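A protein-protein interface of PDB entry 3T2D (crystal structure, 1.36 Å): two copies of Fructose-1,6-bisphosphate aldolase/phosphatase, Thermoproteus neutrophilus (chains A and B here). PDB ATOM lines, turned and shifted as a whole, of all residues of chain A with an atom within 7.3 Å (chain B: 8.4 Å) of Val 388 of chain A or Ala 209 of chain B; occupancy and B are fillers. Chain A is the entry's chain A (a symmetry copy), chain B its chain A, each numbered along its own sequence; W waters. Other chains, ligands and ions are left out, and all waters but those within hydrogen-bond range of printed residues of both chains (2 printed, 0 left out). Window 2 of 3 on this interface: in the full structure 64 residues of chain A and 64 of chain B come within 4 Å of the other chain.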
ATOM      1  N   LYS A 382     -36.474   0.074  16.271  1.00  0.00           N
ATOM      2  CA  LYS A 382     -36.513   0.042  17.706  1.00  0.00           C
ATOM      3  C   LYS A 382     -36.599  -1.320  18.340  1.00  0.00           C
ATOM      4  O   LYS A 382     -35.842  -1.670  19.298  1.00  0.00           O
ATOM      5  CB  LYS A 382     -37.697   0.987  18.191  1.00  0.00           C
ATOM      6  CG  LYS A 382     -37.992   0.867  19.681  1.00  0.00           C
ATOM      7  CD  LYS A 382     -39.166   1.817  20.187  1.00  0.00           C
ATOM      8  CE  LYS A 382     -40.618   1.284  20.001  1.00  0.00           C
ATOM      9  NZ  LYS A 382     -41.700   2.337  20.371  1.00  0.00           N
ATOM     10  N   TYR A 383     -37.443  -2.185  17.757  1.00  0.00           N
ATOM     11  CA  TYR A 383     -37.537  -3.503  18.316  1.00  0.00           C
ATOM     12  C   TYR A 383     -36.301  -4.345  18.125  1.00  0.00           C
ATOM     13  O   TYR A 383     -35.834  -5.059  19.056  1.00  0.00           O
ATOM     14  CB  TYR A 383     -38.697  -4.166  17.670  1.00  0.00           C
ATOM     15  CG  TYR A 383     -40.006  -3.671  18.082  1.00  0.00           C
ATOM     16  CD1 TYR A 383     -40.210  -3.131  19.364  1.00  0.00           C
ATOM     17  CD2 TYR A 383     -40.995  -3.550  17.145  1.00  0.00           C
ATOM     18  CE1 TYR A 383     -41.440  -2.698  19.713  1.00  0.00           C
ATOM     19  CE2 TYR A 383     -42.200  -3.137  17.448  1.00  0.00           C
ATOM     20  CZ  TYR A 383     -42.448  -2.658  18.741  1.00  0.00           C
ATOM     21  OH  TYR A 383     -43.700  -2.181  19.042  1.00  0.00           O
ATOM     22  N   ILE A 384     -35.686  -4.243  16.944  1.00  0.00           N
ATOM     23  CA  ILE A 384     -34.399  -4.929  16.743  1.00  0.00           C
ATOM     24  C   ILE A 384     -33.310  -4.435  17.656  1.00  0.00           C
ATOM     25  O   ILE A 384     -32.586  -5.226  18.238  1.00  0.00           O
ATOM     26  CB  ILE A 384     -33.951  -4.915  15.178  1.00  0.00           C
ATOM     27  CG1 ILE A 384     -35.016  -5.578  14.289  1.00  0.00           C
ATOM     28  CG2 ILE A 384     -32.567  -5.547  15.067  1.00  0.00           C
ATOM     29  CD1 ILE A 384     -35.396  -7.071  14.580  1.00  0.00           C
ATOM     30  N   GLU A 385     -33.183  -3.098  17.857  1.00  0.00           N
ATOM     31  CA  GLU A 385     -32.200  -2.604  18.820  1.00  0.00           C
ATOM     32  C   GLU A 385     -32.480  -3.118  20.196  1.00  0.00           C
ATOM     33  O   GLU A 385     -31.525  -3.468  20.886  1.00  0.00           O
ATOM     34  CB  GLU A 385     -32.139  -1.079  18.857  1.00  0.00           C
ATOM     35  CG  GLU A 385     -31.597  -0.498  17.608  1.00  0.00           C
ATOM     36  CD  GLU A 385     -31.735   1.050  17.481  1.00  0.00           C
ATOM     37  OE1 GLU A 385     -32.203   1.762  18.458  1.00  0.00           O
ATOM     38  OE2 GLU A 385     -31.358   1.546  16.356  1.00  0.00           O
ATOM     39  N   ALA A 386     -33.763  -3.247  20.564  1.00  0.00           N
ATOM     40  CA  ALA A 386     -34.123  -3.745  21.904  1.00  0.00           C
ATOM     41  C   ALA A 386     -33.739  -5.192  22.036  1.00  0.00           C
ATOM     42  O   ALA A 386     -33.146  -5.564  23.024  1.00  0.00           O
ATOM     43  CB  ALA A 386     -35.635  -3.545  22.152  1.00  0.00           C
ATOM     44  N   VAL A 387     -33.917  -6.033  20.981  1.00  0.00           N
ATOM     45  CA  VAL A 387     -33.392  -7.394  21.132  1.00  0.00           C
ATOM     46  C   VAL A 387     -31.871  -7.436  21.228  1.00  0.00           C
ATOM     47  O   VAL A 387     -31.250  -8.262  21.970  1.00  0.00           O
ATOM     48  CB  VAL A 387     -33.775  -8.255  19.933  1.00  0.00           C
ATOM     49  CG1 VAL A 387     -33.071  -9.681  19.993  1.00  0.00           C
ATOM     50  CG2 VAL A 387     -35.281  -8.378  19.846  1.00  0.00           C
ATOM     51  N   VAL A 388     -31.215  -6.638  20.365  1.00  0.00           N
ATOM     52  CA  VAL A 388     -29.775  -6.591  20.333  1.00  0.00           C
ATOM     53  C   VAL A 388     -29.140  -6.204  21.674  1.00  0.00           C
ATOM     54  O   VAL A 388     -28.204  -6.855  22.154  1.00  0.00           O
ATOM     55  CB  VAL A 388     -29.278  -5.696  19.152  1.00  0.00           C
ATOM     56  CG1 VAL A 388     -27.801  -5.489  19.235  1.00  0.00           C
ATOM     57  CG2 VAL A 388     -29.697  -6.333  17.819  1.00  0.00           C
ATOM     58  N   LYS A 389     -29.601  -5.084  22.215  1.00  0.00           N
ATOM     59  CA  LYS A 389     -29.197  -4.588  23.561  1.00  0.00           C
ATOM     60  C   LYS A 389     -29.663  -5.554  24.635  1.00  0.00           C
ATOM     61  O   LYS A 389     -28.862  -6.057  25.481  1.00  0.00           O
ATOM     62  CB  LYS A 389     -29.877  -3.235  23.802  1.00  0.00           C
ATOM     63  CG  LYS A 389     -29.138  -2.082  23.049  1.00  0.00           C
ATOM     64  CD  LYS A 389     -29.619  -0.639  23.466  1.00  0.00           C
ATOM     65  CE  LYS A 389     -29.650   0.363  22.224  1.00  0.00           C
ATOM     66  NZ  LYS A 389     -30.981   1.125  22.119  1.00  0.00           N
ATOM     67  N   GLY A 390     -30.974  -5.797  24.646  1.00  0.00           N
ATOM     68  CA  GLY A 390     -31.498  -6.873  25.470  1.00  0.00           C
ATOM     69  C   GLY A 390     -30.367  -7.893  25.531  1.00  0.00           C
ATOM     70  O   GLY A 390     -30.316  -8.742  26.440  1.00  0.00           O
ATOM     71  N   PRO B 160     -16.496 -18.134  16.443  1.00  0.00           N
ATOM     72  CA  PRO B 160     -16.960 -17.392  17.619  1.00  0.00           C
ATOM     73  C   PRO B 160     -17.755 -16.159  17.286  1.00  0.00           C
ATOM     74  O   PRO B 160     -18.583 -15.737  18.079  1.00  0.00           O
ATOM     75  CB  PRO B 160     -15.658 -17.087  18.347  1.00  0.00           C
ATOM     76  CG  PRO B 160     -14.603 -17.242  17.402  1.00  0.00           C
ATOM     77  CD  PRO B 160     -15.036 -18.222  16.366  1.00  0.00           C
ATOM     78  N   SER B 161     -17.563 -15.575  16.125  1.00  0.00           N
ATOM     79  CA  SER B 161     -18.352 -14.407  15.755  1.00  0.00           C
ATOM     80  C   SER B 161     -19.789 -14.637  15.512  1.00  0.00           C
ATOM     81  O   SER B 161     -20.549 -13.694  15.412  1.00  0.00           O
ATOM     82  CB  SER B 161     -17.700 -13.682  14.530  1.00  0.00           C
ATOM     83  OG  SER B 161     -17.900 -14.368  13.339  1.00  0.00           O
ATOM     84  N   MET B 162     -20.220 -15.921  15.370  1.00  0.00           N
ATOM     85  CA  MET B 162     -21.601 -16.292  15.094  1.00  0.00           C
ATOM     86  C   MET B 162     -22.334 -16.912  16.294  1.00  0.00           C
ATOM     87  O   MET B 162     -23.493 -17.292  16.181  1.00  0.00           O
ATOM     88  CB  MET B 162     -21.651 -17.347  13.933  1.00  0.00           C
ATOM     89  CG  MET B 162     -21.070 -16.779  12.667  1.00  0.00           C
ATOM     90  SD  MET B 162     -21.171 -17.786  11.193  1.00  0.00           S
ATOM     91  CE  MET B 162     -22.925 -17.850  10.932  1.00  0.00           C
ATOM     92  N   HIS B 163     -21.659 -16.976  17.415  1.00  0.00           N
ATOM     93  CA  HIS B 163     -22.107 -17.805  18.498  1.00  0.00           C
ATOM     94  C   HIS B 163     -23.452 -17.265  19.035  1.00  0.00           C
ATOM     95  O   HIS B 163     -24.230 -18.012  19.648  1.00  0.00           O
ATOM     96  CB  HIS B 163     -21.063 -17.723  19.629  1.00  0.00           C
ATOM     97  CG  HIS B 163     -21.214 -18.778  20.674  1.00  0.00           C
ATOM     98  ND1 HIS B 163     -21.779 -18.496  21.894  1.00  0.00           N
ATOM     99  CD2 HIS B 163     -20.862 -20.093  20.696  1.00  0.00           C
ATOM    100  CE1 HIS B 163     -21.831 -19.615  22.611  1.00  0.00           C
ATOM    101  NE2 HIS B 163     -21.294 -20.600  21.891  1.00  0.00           N
ATOM    102  N   GLU B 164     -23.682 -15.957  18.923  1.00  0.00           N
ATOM    103  CA  GLU B 164     -24.875 -15.370  19.482  1.00  0.00           C
ATOM    104  C   GLU B 164     -26.153 -15.534  18.700  1.00  0.00           C
ATOM    105  O   GLU B 164     -27.242 -15.253  19.188  1.00  0.00           O
ATOM    106  CB  GLU B 164     -24.691 -13.896  19.779  1.00  0.00           C
ATOM    107  CG  GLU B 164     -23.648 -13.677  20.948  1.00  0.00           C
ATOM    108  CD  GLU B 164     -22.152 -13.835  20.609  1.00  0.00           C
ATOM    109  OE1 GLU B 164     -21.351 -14.361  21.546  1.00  0.00           O
ATOM    110  OE2 GLU B 164     -21.762 -13.348  19.473  1.00  0.00           O
ATOM    111  N   GLY B 165     -26.032 -16.021  17.472  1.00  0.00           N
ATOM    112  CA  GLY B 165     -27.217 -16.375  16.728  1.00  0.00           C
ATOM    113  C   GLY B 165     -27.891 -15.248  16.006  1.00  0.00           C
ATOM    114  O   GLY B 165     -27.305 -14.203  15.638  1.00  0.00           O
ATOM    115  N   PHE B 166     -29.159 -15.463  15.685  1.00  0.00           N
ATOM    116  CA  PHE B 166     -29.881 -14.663  14.761  1.00  0.00           C
ATOM    117  C   PHE B 166     -31.299 -14.308  15.260  1.00  0.00           C
ATOM    118  O   PHE B 166     -31.856 -15.019  16.118  1.00  0.00           O
ATOM    119  CB  PHE B 166     -29.946 -15.324  13.330  1.00  0.00           C
ATOM    120  CG  PHE B 166     -28.589 -15.281  12.687  1.00  0.00           C
ATOM    121  CD1 PHE B 166     -27.658 -16.258  12.894  1.00  0.00           C
ATOM    122  CD2 PHE B 166     -28.236 -14.194  11.856  1.00  0.00           C
ATOM    123  CE1 PHE B 166     -26.388 -16.177  12.378  1.00  0.00           C
ATOM    124  CE2 PHE B 166     -26.975 -14.109  11.342  1.00  0.00           C
ATOM    125  CZ  PHE B 166     -26.035 -15.102  11.629  1.00  0.00           C
ATOM    126  N   ILE B 167     -31.872 -13.264  14.681  1.00  0.00           N
ATOM    127  CA  ILE B 167     -33.212 -12.806  14.966  1.00  0.00           C
ATOM    128  C   ILE B 167     -34.044 -12.967  13.731  1.00  0.00           C
ATOM    129  O   ILE B 167     -33.731 -12.509  12.644  1.00  0.00           O
ATOM    130  CB  ILE B 167     -33.236 -11.300  15.342  1.00  0.00           C
ATOM    131  CG1 ILE B 167     -32.239 -10.969  16.474  1.00  0.00           C
ATOM    132  CG2 ILE B 167     -34.644 -10.916  15.705  1.00  0.00           C
ATOM    133  CD1 ILE B 167     -31.960  -9.435  16.677  1.00  0.00           C
ATOM    134  N   LEU B 180     -40.965 -11.810  16.596  1.00  0.00           N
ATOM    135  CA  LEU B 180     -39.543 -11.753  16.594  1.00  0.00           C
ATOM    136  C   LEU B 180     -39.002 -12.842  17.471  1.00  0.00           C
ATOM    137  O   LEU B 180     -39.302 -12.954  18.696  1.00  0.00           O
ATOM    138  CB  LEU B 180     -39.052 -10.441  17.147  1.00  0.00           C
ATOM    139  CG  LEU B 180     -39.200  -9.321  16.262  1.00  0.00           C
ATOM    140  CD1 LEU B 180     -38.678  -8.014  17.030  1.00  0.00           C
ATOM    141  CD2 LEU B 180     -38.357  -9.440  14.902  1.00  0.00           C
ATOM    142  N   LYS B 182     -35.567 -15.383  18.533  1.00  0.00           N
ATOM    143  CA  LYS B 182     -34.140 -15.409  18.569  1.00  0.00           C
ATOM    144  C   LYS B 182     -33.601 -16.802  18.721  1.00  0.00           C
ATOM    145  O   LYS B 182     -34.000 -17.480  19.668  1.00  0.00           O
ATOM    146  CB  LYS B 182     -33.630 -14.555  19.767  1.00  0.00           C
ATOM    147  CG  LYS B 182     -34.083 -13.150  19.709  1.00  0.00           C
ATOM    148  CD  LYS B 182     -35.026 -12.828  20.794  1.00  0.00           C
ATOM    149  CE  LYS B 182     -34.268 -12.985  22.081  1.00  0.00           C
ATOM    150  NZ  LYS B 182     -34.950 -12.649  23.387  1.00  0.00           N
ATOM    151  N   PHE B 206     -31.933 -10.948  10.989  1.00  0.00           N
ATOM    152  CA  PHE B 206     -30.928  -9.993  11.422  1.00  0.00           C
ATOM    153  C   PHE B 206     -29.921 -10.718  12.304  1.00  0.00           C
ATOM    154  O   PHE B 206     -30.248 -11.638  13.060  1.00  0.00           O
ATOM    155  CB  PHE B 206     -31.611  -8.825  12.236  1.00  0.00           C
ATOM    156  CG  PHE B 206     -32.633  -8.106  11.498  1.00  0.00           C
ATOM    157  CD1 PHE B 206     -32.330  -7.039  10.718  1.00  0.00           C
ATOM    158  CD2 PHE B 206     -33.973  -8.530  11.550  1.00  0.00           C
ATOM    159  CE1 PHE B 206     -33.315  -6.361   9.995  1.00  0.00           C
ATOM    160  CE2 PHE B 206     -34.932  -7.894  10.816  1.00  0.00           C
ATOM    161  CZ  PHE B 206     -34.646  -6.836  10.043  1.00  0.00           C
ATOM    162  N   ARG B 207     -28.675 -10.270  12.232  1.00  0.00           N
ATOM    163  CA  ARG B 207     -27.671 -10.776  13.106  1.00  0.00           C
ATOM    164  C   ARG B 207     -27.948 -10.282  14.550  1.00  0.00           C
ATOM    165  O   ARG B 207     -28.199  -9.104  14.788  1.00  0.00           O
ATOM    166  CB  ARG B 207     -26.289 -10.282  12.612  1.00  0.00           C
ATOM    167  CG  ARG B 207     -25.330 -10.773  13.480  1.00  0.00           C
ATOM    168  CD  ARG B 207     -24.255 -11.043  12.912  1.00  0.00           C
ATOM    169  NE  ARG B 207     -23.483 -10.121  12.438  1.00  0.00           N
ATOM    170  CZ  ARG B 207     -22.114 -10.184  12.713  1.00  0.00           C
ATOM    171  NH1 ARG B 207     -21.260  -9.291  12.263  1.00  0.00           N
ATOM    172  NH2 ARG B 207     -21.529 -11.083  13.530  1.00  0.00           N
ATOM    173  N   ARG B 208     -27.891 -11.176  15.535  1.00  0.00           N
ATOM    174  CA  ARG B 208     -28.131 -10.798  16.893  1.00  0.00           C
ATOM    175  C   ARG B 208     -27.007  -9.898  17.478  1.00  0.00           C
ATOM    176  O   ARG B 208     -27.340  -9.003  18.317  1.00  0.00           O
ATOM    177  CB  ARG B 208     -28.326 -11.997  17.814  1.00  0.00           C
ATOM    178  CG  ARG B 208     -28.453 -11.618  19.175  1.00  0.00           C
ATOM    179  CD  ARG B 208     -29.573 -11.858  19.917  1.00  0.00           C
ATOM    180  NE  ARG B 208     -29.648 -13.286  20.053  1.00  0.00           N
ATOM    181  CZ  ARG B 208     -30.133 -14.123  20.976  1.00  0.00           C
ATOM    182  NH1 ARG B 208     -30.445 -13.783  22.148  1.00  0.00           N
ATOM    183  NH2 ARG B 208     -30.160 -15.447  20.664  1.00  0.00           N
ATOM    184  N   ALA B 209     -25.783 -10.072  17.058  1.00  0.00           N
ATOM    185  CA  ALA B 209     -24.648  -9.362  17.693  1.00  0.00           C
ATOM    186  C   ALA B 209     -24.792  -7.875  17.513  1.00  0.00           C
ATOM    187  O   ALA B 209     -24.458  -7.098  18.420  1.00  0.00           O
ATOM    188  CB  ALA B 209     -23.367  -9.819  17.086  1.00  0.00           C
ATOM    189  N   ASP B 210     -25.269  -7.438  16.361  1.00  0.00           N
ATOM    190  CA  ASP B 210     -25.313  -6.020  16.031  1.00  0.00           C
ATOM    191  C   ASP B 210     -26.583  -5.559  15.332  1.00  0.00           C
ATOM    192  O   ASP B 210     -26.709  -4.377  14.956  1.00  0.00           O
ATOM    193  CB  ASP B 210     -24.131  -5.621  15.195  1.00  0.00           C
ATOM    194  CG  ASP B 210     -24.055  -6.266  13.821  1.00  0.00           C
ATOM    195  OD1 ASP B 210     -24.878  -7.161  13.530  1.00  0.00           O
ATOM    196  OD2 ASP B 210     -23.152  -5.878  13.006  1.00  0.00           O
ATOM    197  N   GLY B 211     -27.545  -6.462  15.065  1.00  0.00           N
ATOM    198  CA  GLY B 211     -28.706  -6.116  14.355  1.00  0.00           C
ATOM    199  C   GLY B 211     -28.589  -5.992  12.835  1.00  0.00           C
ATOM    200  O   GLY B 211     -29.547  -5.529  12.194  1.00  0.00           O
ATOM    201  N   ALA B 212     -27.447  -6.360  12.255  1.00  0.00           N
ATOM    202  CA  ALA B 212     -27.214  -6.210  10.813  1.00  0.00           C
ATOM    203  C   ALA B 212     -28.257  -7.023  10.003  1.00  0.00           C
ATOM    204  O   ALA B 212     -28.560  -8.171  10.341  1.00  0.00           O
ATOM    205  CB  ALA B 212     -25.850  -6.744  10.410  1.00  0.00           C
ATOM    206  N   GLY B 244     -19.188 -13.494   9.737  1.00  0.00           N
ATOM    207  CA  GLY B 244     -20.183 -13.531  10.777  1.00  0.00           C
ATOM    208  C   GLY B 244     -21.588 -13.767  10.298  1.00  0.00           C
ATOM    209  O   GLY B 244     -22.487 -14.069  11.106  1.00  0.00           O
HETATM  210  O   HOH W   1     -33.685  -9.920  23.713  1.00  0.00           O
HETATM  211  O   HOH W   2     -27.133  -9.048  21.031  1.00  0.00           O
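Of the 9 printed residues of chain A, 4 touch a printed residue of chain B.
Printed residues of chain A that touch a printed residue of chain B: Tyr 383, Ile 384, Val 387 and Val 388.
Hydrophobic or aromatic side chains of chain A that line the printed part of chain B: Tyr 383, Ile 384, Val 387 and Val 388.
Of the 18 printed residues of chain B, 7 touch a printed residue of chain A.
Hydrophobic or aromatic side chains of chain B that line the printed part of chain A: Ile 167, Leu 180 and Phe 206.
Among the printed residues, no Asp or Glu carboxylate lies within 4 Å of a Lys or Arg side-chain nitrogen of the other chain.
NE of Arg 208 of chain B sits at hydrogen-bond distance from O of Glu 164 of chain B (3.2 Å).
O of Gly 165 of chain B lies within hydrogen-bond range of N of Arg 208 of chain B (3.1 Å).
N of Ile 167 of chain B lies within hydrogen-bond range of O of Phe 206 of chain B, at 2.8 Å.
Leu 180 of chain B touches Tyr 383 of chain A (CD1 to CB, 3.9 Å).
CD2 of Leu 180 of chain B touches CD1 of Ile 384 of chain A (3.8 Å).
Phe 206 of chain B touches Ile 384 of chain A.
Ile 384 of chain A touches Gly 211 of chain B.
Ile 167 of chain B touches Val 387 of chain A (CD1 to CG1, 3.5 Å).
Val 387 of chain A touches Lys 182 of chain B (CG1 to CG, 3.6 Å).
CG2 of Val 388 of chain A touches O of Arg 208 of chain B, at 3.6 Å.
Ala 209 of chain B touches Val 388 of chain A (O to CG1, 3.8 Å).
N of Gly 211 of chain B touches CG2 of Val 388 of chain A, 3.5 Å away.
Water W2 bridges the backbone carbonyl oxygen (O) of Val 388 of chain A (2.7 Å) and the backbone carbonyl oxygen (O) of Arg 208 of chain B (2.7 Å).
Water W1 lies within hydrogen-bond range of the side-chain amino group of Lys 182 of chain B (3.0 Å) and the backbone carbonyl oxygen of Val 387 of chain A (3.4 Å).
Ala 209 of chain B touches just one residue of chain A: Val 388 (3.8 Å).
Of the printed residues of chain A, Arg 208 of chain B touches Val 388 (3.6 Å).
Printed residues of chain B within 4 Å of Val 387 of chain A: Ile 167 and Lys 182.
Gly 244 of chain B touches none of the printed residues of chain A.
The nearest printed residue of chain B that does not touch Val 388 of chain A is Ile 167 of chain B (4.01 Å).
The nearest residue of chain A that does not touch Ala 209 of chain B is Lys 389 of chain A (6.7 Å).
No position is printed for both chains.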
